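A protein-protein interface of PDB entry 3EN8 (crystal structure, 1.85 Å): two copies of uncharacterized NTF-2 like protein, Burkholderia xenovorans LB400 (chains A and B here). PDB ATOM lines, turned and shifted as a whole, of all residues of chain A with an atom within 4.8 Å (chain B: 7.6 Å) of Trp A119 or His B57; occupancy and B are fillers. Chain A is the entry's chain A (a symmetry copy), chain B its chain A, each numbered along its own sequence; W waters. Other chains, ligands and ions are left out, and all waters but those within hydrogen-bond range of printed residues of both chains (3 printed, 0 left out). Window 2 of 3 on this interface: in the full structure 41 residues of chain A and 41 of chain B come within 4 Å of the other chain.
OE1 of Glu B43 lies within salt-bridge range of NH2 of Arg A120 (2.7 Å).
Pro A117 touches Glu B43 (CD to OE2, 3.3 Å).
Trp A119 touches Leu B54.
ND1 of His B57 touches CZ3 of Trp A119, 3.0 Å away.
Trp A119 touches His B58 (CZ2 to O, 3.5 Å).
CB of Arg A120 touches CD2 of Leu B54, 3.8 Å away.
Trp A123 touches Leu B54.
Of the printed residues of chain B, Pro A117 touches Glu B43.
No residue of chain B comes within 4 Å of Gly A118.
Of chain B, only Leu B54 (3.4 Å), His B57 (3.0 Å) and His B58 (3.5 Å) come within 4 Å of Trp A119.
His B57 touches just one residue of chain A: Trp A119.
Printed residues of chain A within 4 Å of His B58: Trp A119 (3.5 Å).
The nearest printed residue of chain A that does not touch His B57 is Trp A123 (6.6 Å).
The nearest printed residue of chain B that does not touch Pro A117 is His B58 (6.8 Å).
Of the 6 printed residues of chain A, 4 touch a printed residue of chain B.
Hydrophobic or aromatic side chains of chain A that line the printed part of chain B: Pro A117, Trp A119 and Trp A123.
Of the 14 printed residues of chain B, 4 touch a printed residue of chain A.
Hydrophobic or aromatic side chains of chain B that line the printed part of chain A: Leu B54, His B57 and His B58.
No position is printed for both chains.
Of the 7 pairs that touch across the chains among the printed residues, none has its exchanged pair printed and touching as well.
Water W3 lies within hydrogen-bond range of the backbone carbonyl oxygen (O) of Trp A123 and the side-chain amide nitrogen (ND2) of Asn B50.
Water W2 lies within hydrogen-bond range of O of Pro A117 (2.7 Å), OE2 of Glu B43 (2.7 Å) and N of Ser A121 (3.4 Å).
Water W1 lies within hydrogen-bond range of the backbone carbonyl oxygen (O) of His B58, the guanidinium group (NH1) of Arg A120 and the backbone carbonyl oxygen (O) of Leu B54.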
ATOM      1  N   PRO A 117     -20.460  31.922  19.783  1.00  0.00           N
ATOM      2  CA  PRO A 117     -20.480  32.997  18.789  1.00  0.00           C
ATOM      3  C   PRO A 117     -21.844  33.173  18.163  1.00  0.00           C
ATOM      4  O   PRO A 117     -22.588  32.214  17.985  1.00  0.00           O
ATOM      5  CB  PRO A 117     -19.452  32.543  17.739  1.00  0.00           C
ATOM      6  CG  PRO A 117     -18.852  31.246  18.261  1.00  0.00           C
ATOM      7  CD  PRO A 117     -19.809  30.710  19.258  1.00  0.00           C
ATOM      8  N   GLY A 118     -22.171  34.426  17.885  1.00  0.00           N
ATOM      9  CA  GLY A 118     -23.492  34.783  17.402  1.00  0.00           C
ATOM     10  C   GLY A 118     -23.832  34.115  16.095  1.00  0.00           C
ATOM     11  O   GLY A 118     -24.967  33.698  15.878  1.00  0.00           O
ATOM     12  N   TRP A 119     -22.828  33.972  15.246  1.00  0.00           N
ATOM     13  CA  TRP A 119     -23.071  33.556  13.864  1.00  0.00           C
ATOM     14  C   TRP A 119     -23.754  32.212  13.755  1.00  0.00           C
ATOM     15  O   TRP A 119     -24.555  31.986  12.836  1.00  0.00           O
ATOM     16  CB  TRP A 119     -21.786  33.574  13.010  1.00  0.00           C
ATOM     17  CG  TRP A 119     -20.771  32.475  13.270  1.00  0.00           C
ATOM     18  CD1 TRP A 119     -19.708  32.533  14.130  1.00  0.00           C
ATOM     19  CD2 TRP A 119     -20.687  31.195  12.622  1.00  0.00           C
ATOM     20  NE1 TRP A 119     -18.989  31.370  14.076  1.00  0.00           N
ATOM     21  CE2 TRP A 119     -19.567  30.528  13.162  1.00  0.00           C
ATOM     22  CE3 TRP A 119     -21.456  30.545  11.653  1.00  0.00           C
ATOM     23  CZ2 TRP A 119     -19.195  29.241  12.764  1.00  0.00           C
ATOM     24  CZ3 TRP A 119     -21.080  29.257  11.255  1.00  0.00           C
ATOM     25  CH2 TRP A 119     -19.964  28.624  11.815  1.00  0.00           C
ATOM     26  N   ARG A 120     -23.445  31.325  14.693  1.00  0.00           N
ATOM     27  CA  ARG A 120     -23.950  29.941  14.637  1.00  0.00           C
ATOM     28  C   ARG A 120     -25.064  29.690  15.651  1.00  0.00           C
ATOM     29  O   ARG A 120     -25.516  28.579  15.845  1.00  0.00           O
ATOM     30  CB  ARG A 120     -22.823  28.914  14.786  1.00  0.00           C
ATOM     31  CG  ARG A 120     -21.975  29.016  16.037  1.00  0.00           C
ATOM     32  CD  ARG A 120     -21.074  27.778  16.167  1.00  0.00           C
ATOM     33  NE  ARG A 120     -20.355  27.764  17.429  1.00  0.00           N
ATOM     34  CZ  ARG A 120     -19.030  27.742  17.519  1.00  0.00           C
ATOM     35  NH1 ARG A 120     -18.295  27.666  16.422  1.00  0.00           N
ATOM     36  NH2 ARG A 120     -18.444  27.770  18.708  1.00  0.00           N
ATOM     37  N   SER A 121     -25.541  30.767  16.249  1.00  0.00           N
ATOM     38  CA  SER A 121     -26.559  30.678  17.306  1.00  0.00           C
ATOM     39  C   SER A 121     -27.795  29.920  16.842  1.00  0.00           C
ATOM     40  O   SER A 121     -28.400  29.141  17.601  1.00  0.00           O
ATOM     41  CB  SER A 121     -26.972  32.077  17.785  1.00  0.00           C
ATOM     42  OG  SER A 121     -27.663  32.782  16.766  1.00  0.00           O
ATOM     43  N   TRP A 123     -28.076  27.652  15.008  1.00  0.00           N
ATOM     44  CA  TRP A 123     -27.752  26.251  14.665  1.00  0.00           C
ATOM     45  C   TRP A 123     -27.232  25.459  15.842  1.00  0.00           C
ATOM     46  O   TRP A 123     -26.890  24.282  15.723  1.00  0.00           O
ATOM     47  CB  TRP A 123     -26.761  26.180  13.499  1.00  0.00           C
ATOM     48  CG  TRP A 123     -27.388  26.659  12.236  1.00  0.00           C
ATOM     49  CD1 TRP A 123     -28.384  26.047  11.536  1.00  0.00           C
ATOM     50  CD2 TRP A 123     -27.078  27.867  11.527  1.00  0.00           C
ATOM     51  NE1 TRP A 123     -28.724  26.804  10.426  1.00  0.00           N
ATOM     52  CE2 TRP A 123     -27.933  27.924  10.400  1.00  0.00           C
ATOM     53  CE3 TRP A 123     -26.173  28.909  11.742  1.00  0.00           C
ATOM     54  CZ2 TRP A 123     -27.896  28.981   9.484  1.00  0.00           C
ATOM     55  CZ3 TRP A 123     -26.130  29.949  10.831  1.00  0.00           C
ATOM     56  CH2 TRP A 123     -26.991  29.982   9.716  1.00  0.00           C
ATOM     57  N   PHE B  23     -14.199  17.876   3.945  1.00  0.00           N
ATOM     58  CA  PHE B  23     -15.270  17.981   4.953  1.00  0.00           C
ATOM     59  C   PHE B  23     -16.222  16.812   4.847  1.00  0.00           C
ATOM     60  O   PHE B  23     -16.798  16.380   5.841  1.00  0.00           O
ATOM     61  CB  PHE B  23     -16.031  19.301   4.841  1.00  0.00           C
ATOM     62  CG  PHE B  23     -15.153  20.503   5.010  1.00  0.00           C
ATOM     63  CD1 PHE B  23     -14.593  20.793   6.234  1.00  0.00           C
ATOM     64  CD2 PHE B  23     -14.882  21.330   3.948  1.00  0.00           C
ATOM     65  CE1 PHE B  23     -13.759  21.900   6.382  1.00  0.00           C
ATOM     66  CE2 PHE B  23     -14.058  22.433   4.101  1.00  0.00           C
ATOM     67  CZ  PHE B  23     -13.505  22.705   5.326  1.00  0.00           C
ATOM     68  N   GLU B  43     -22.290  25.126  24.123  1.00  0.00           N
ATOM     69  CA  GLU B  43     -22.940  24.897  22.822  1.00  0.00           C
ATOM     70  C   GLU B  43     -23.030  23.413  22.517  1.00  0.00           C
ATOM     71  O   GLU B  43     -22.098  22.640  22.791  1.00  0.00           O
ATOM     72  CB  GLU B  43     -22.201  25.577  21.680  1.00  0.00           C
ATOM     73  CG  GLU B  43     -22.178  27.052  21.773  1.00  0.00           C
ATOM     74  CD  GLU B  43     -21.323  27.649  20.710  1.00  0.00           C
ATOM     75  OE1 GLU B  43     -20.093  27.652  20.897  1.00  0.00           O
ATOM     76  OE2 GLU B  43     -21.871  28.143  19.698  1.00  0.00           O
ATOM     77  N   ASN B  50     -25.464  19.372  10.123  1.00  0.00           N
ATOM     78  CA  ASN B  50     -25.287  20.699  10.756  1.00  0.00           C
ATOM     79  C   ASN B  50     -23.837  20.858  11.161  1.00  0.00           C
ATOM     80  O   ASN B  50     -23.242  21.911  10.971  1.00  0.00           O
ATOM     81  CB  ASN B  50     -26.213  20.928  11.971  1.00  0.00           C
ATOM     82  CG  ASN B  50     -27.585  21.451  11.568  1.00  0.00           C
ATOM     83  OD1 ASN B  50     -27.845  21.719  10.390  1.00  0.00           O
ATOM     84  ND2 ASN B  50     -28.467  21.600  12.545  1.00  0.00           N
ATOM     85  N   LEU B  51     -23.272  19.769  11.688  1.00  0.00           N
ATOM     86  CA  LEU B  51     -21.885  19.781  12.175  1.00  0.00           C
ATOM     87  C   LEU B  51     -20.923  20.079  11.023  1.00  0.00           C
ATOM     88  O   LEU B  51     -20.038  20.921  11.120  1.00  0.00           O
ATOM     89  CB  LEU B  51     -21.523  18.437  12.837  1.00  0.00           C
ATOM     90  CG  LEU B  51     -20.169  18.393  13.535  1.00  0.00           C
ATOM     91  CD1 LEU B  51     -20.056  19.457  14.636  1.00  0.00           C
ATOM     92  CD2 LEU B  51     -19.935  16.964  14.065  1.00  0.00           C
ATOM     93  N   GLN B  52     -21.171  19.428   9.902  1.00  0.00           N
ATOM     94  CA  GLN B  52     -20.306  19.579   8.731  1.00  0.00           C
ATOM     95  C   GLN B  52     -20.396  20.989   8.152  1.00  0.00           C
ATOM     96  O   GLN B  52     -19.385  21.586   7.752  1.00  0.00           O
ATOM     97  CB  GLN B  52     -20.647  18.564   7.656  1.00  0.00           C
ATOM     98  CG  GLN B  52     -19.884  18.795   6.371  1.00  0.00           C
ATOM     99  CD  GLN B  52     -19.946  17.627   5.401  1.00  0.00           C
ATOM    100  OE1 GLN B  52     -20.381  16.510   5.734  1.00  0.00           O
ATOM    101  NE2 GLN B  52     -19.509  17.887   4.189  1.00  0.00           N
ATOM    102  N   ALA B  53     -21.617  21.501   8.088  1.00  0.00           N
ATOM    103  CA  ALA B  53     -21.869  22.802   7.463  1.00  0.00           C
ATOM    104  C   ALA B  53     -21.237  23.879   8.315  1.00  0.00           C
ATOM    105  O   ALA B  53     -20.607  24.823   7.817  1.00  0.00           O
ATOM    106  CB  ALA B  53     -23.377  23.063   7.284  1.00  0.00           C
ATOM    107  N   LEU B  54     -21.361  23.706   9.622  1.00  0.00           N
ATOM    108  CA  LEU B  54     -20.848  24.711  10.558  1.00  0.00           C
ATOM    109  C   LEU B  54     -19.329  24.721  10.484  1.00  0.00           C
ATOM    110  O   LEU B  54     -18.709  25.780  10.379  1.00  0.00           O
ATOM    111  CB  LEU B  54     -21.350  24.483  11.988  1.00  0.00           C
ATOM    112  CG  LEU B  54     -22.820  24.840  12.230  1.00  0.00           C
ATOM    113  CD1 LEU B  54     -23.270  24.382  13.635  1.00  0.00           C
ATOM    114  CD2 LEU B  54     -23.091  26.353  12.007  1.00  0.00           C
ATOM    115  N   ARG B  55     -18.729  23.532  10.472  1.00  0.00           N
ATOM    116  CA  ARG B  55     -17.255  23.444  10.454  1.00  0.00           C
ATOM    117  C   ARG B  55     -16.688  23.975   9.136  1.00  0.00           C
ATOM    118  O   ARG B  55     -15.620  24.597   9.093  1.00  0.00           O
ATOM    119  CB  ARG B  55     -16.765  22.016  10.693  1.00  0.00           C
ATOM    120  CG  ARG B  55     -16.831  21.605  12.180  1.00  0.00           C
ATOM    121  CD  ARG B  55     -16.602  20.112  12.343  1.00  0.00           C
ATOM    122  NE  ARG B  55     -16.502  19.699  13.733  1.00  0.00           N
ATOM    123  CZ  ARG B  55     -16.480  18.424  14.097  1.00  0.00           C
ATOM    124  NH1 ARG B  55     -16.565  17.496  13.177  1.00  0.00           N
ATOM    125  NH2 ARG B  55     -16.333  18.091  15.368  1.00  0.00           N
ATOM    126  N   SER B  56     -17.446  23.742   8.076  1.00  0.00           N
ATOM    127  CA  SER B  56     -16.981  24.033   6.706  1.00  0.00           C
ATOM    128  C   SER B  56     -16.996  25.524   6.486  1.00  0.00           C
ATOM    129  O   SER B  56     -16.271  26.078   5.645  1.00  0.00           O
ATOM    130  CB  SER B  56     -17.873  23.367   5.658  1.00  0.00           C
ATOM    131  OG  SER B  56     -17.514  22.015   5.514  1.00  0.00           O
ATOM    132  N   HIS B  57     -17.851  26.151   7.265  1.00  0.00           N
ATOM    133  CA  HIS B  57     -18.149  27.573   7.138  1.00  0.00           C
ATOM    134  C   HIS B  57     -17.086  28.356   7.862  1.00  0.00           C
ATOM    135  O   HIS B  57     -16.480  29.305   7.347  1.00  0.00           O
ATOM    136  CB  HIS B  57     -19.504  27.894   7.782  1.00  0.00           C
ATOM    137  CG  HIS B  57     -19.900  29.330   7.650  1.00  0.00           C
ATOM    138  ND1 HIS B  57     -19.810  30.228   8.694  1.00  0.00           N
ATOM    139  CD2 HIS B  57     -20.344  30.035   6.585  1.00  0.00           C
ATOM    140  CE1 HIS B  57     -20.207  31.420   8.280  1.00  0.00           C
ATOM    141  NE2 HIS B  57     -20.534  31.330   7.004  1.00  0.00           N
ATOM    142  N   HIS B  58     -16.919  27.955   9.105  1.00  0.00           N
ATOM    143  CA  HIS B  58     -15.903  28.537   9.980  1.00  0.00           C
ATOM    144  C   HIS B  58     -15.593  27.654  11.183  1.00  0.00           C
ATOM    145  O   HIS B  58     -16.510  27.220  11.881  1.00  0.00           O
ATOM    146  CB  HIS B  58     -16.351  29.919  10.448  1.00  0.00           C
ATOM    147  CG  HIS B  58     -15.363  30.588  11.345  1.00  0.00           C
ATOM    148  ND1 HIS B  58     -14.464  31.529  10.890  1.00  0.00           N
ATOM    149  CD2 HIS B  58     -15.101  30.421  12.664  1.00  0.00           C
ATOM    150  CE1 HIS B  58     -13.705  31.928  11.894  1.00  0.00           C
ATOM    151  NE2 HIS B  58     -14.073  31.275  12.983  1.00  0.00           N
ATOM    152  N   PRO B  59     -14.291  27.433  11.469  1.00  0.00           N
ATOM    153  CA  PRO B  59     -13.147  28.138  10.873  1.00  0.00           C
ATOM    154  C   PRO B  59     -12.641  27.552   9.555  1.00  0.00           C
ATOM    155  O   PRO B  59     -11.700  28.061   8.951  1.00  0.00           O
ATOM    156  CB  PRO B  59     -12.064  27.993  11.952  1.00  0.00           C
ATOM    157  CG  PRO B  59     -12.354  26.674  12.588  1.00  0.00           C
ATOM    158  CD  PRO B  59     -13.865  26.477  12.508  1.00  0.00           C
ATOM    159  N   GLY B  60     -13.297  26.500   9.103  1.00  0.00           N
ATOM    160  CA  GLY B  60     -12.863  25.805   7.887  1.00  0.00           C
ATOM    161  C   GLY B  60     -11.578  25.034   8.103  1.00  0.00           C
ATOM    162  O   GLY B  60     -11.199  24.751   9.224  1.00  0.00           O
ATOM    163  N   LYS B  61     -10.901  24.722   7.010  1.00  0.00           N
ATOM    164  CA  LYS B  61      -9.683  23.906   7.059  1.00  0.00           C
ATOM    165  C   LYS B  61      -8.570  24.559   7.893  1.00  0.00           C
ATOM    166  O   LYS B  61      -8.227  25.722   7.681  1.00  0.00           O
ATOM    167  CB  LYS B  61      -9.162  23.653   5.644  1.00  0.00           C
ATOM    168  CG  LYS B  61      -7.977  22.710   5.597  1.00  0.00           C
ATOM    169  CD  LYS B  61      -7.234  22.863   4.313  1.00  0.00           C
ATOM    170  CE  LYS B  61      -5.928  22.109   4.335  1.00  0.00           C
ATOM    171  NZ  LYS B  61      -5.263  22.237   3.014  1.00  0.00           N
HETATM  172  O   HOH W   1     -18.540  26.350  13.719  1.00  0.00           O
HETATM  173  O   HOH W   2     -23.736  30.020  19.009  1.00  0.00           O
HETATM  174  O   HOH W   3     -27.776  21.894  15.838  1.00  0.00           O
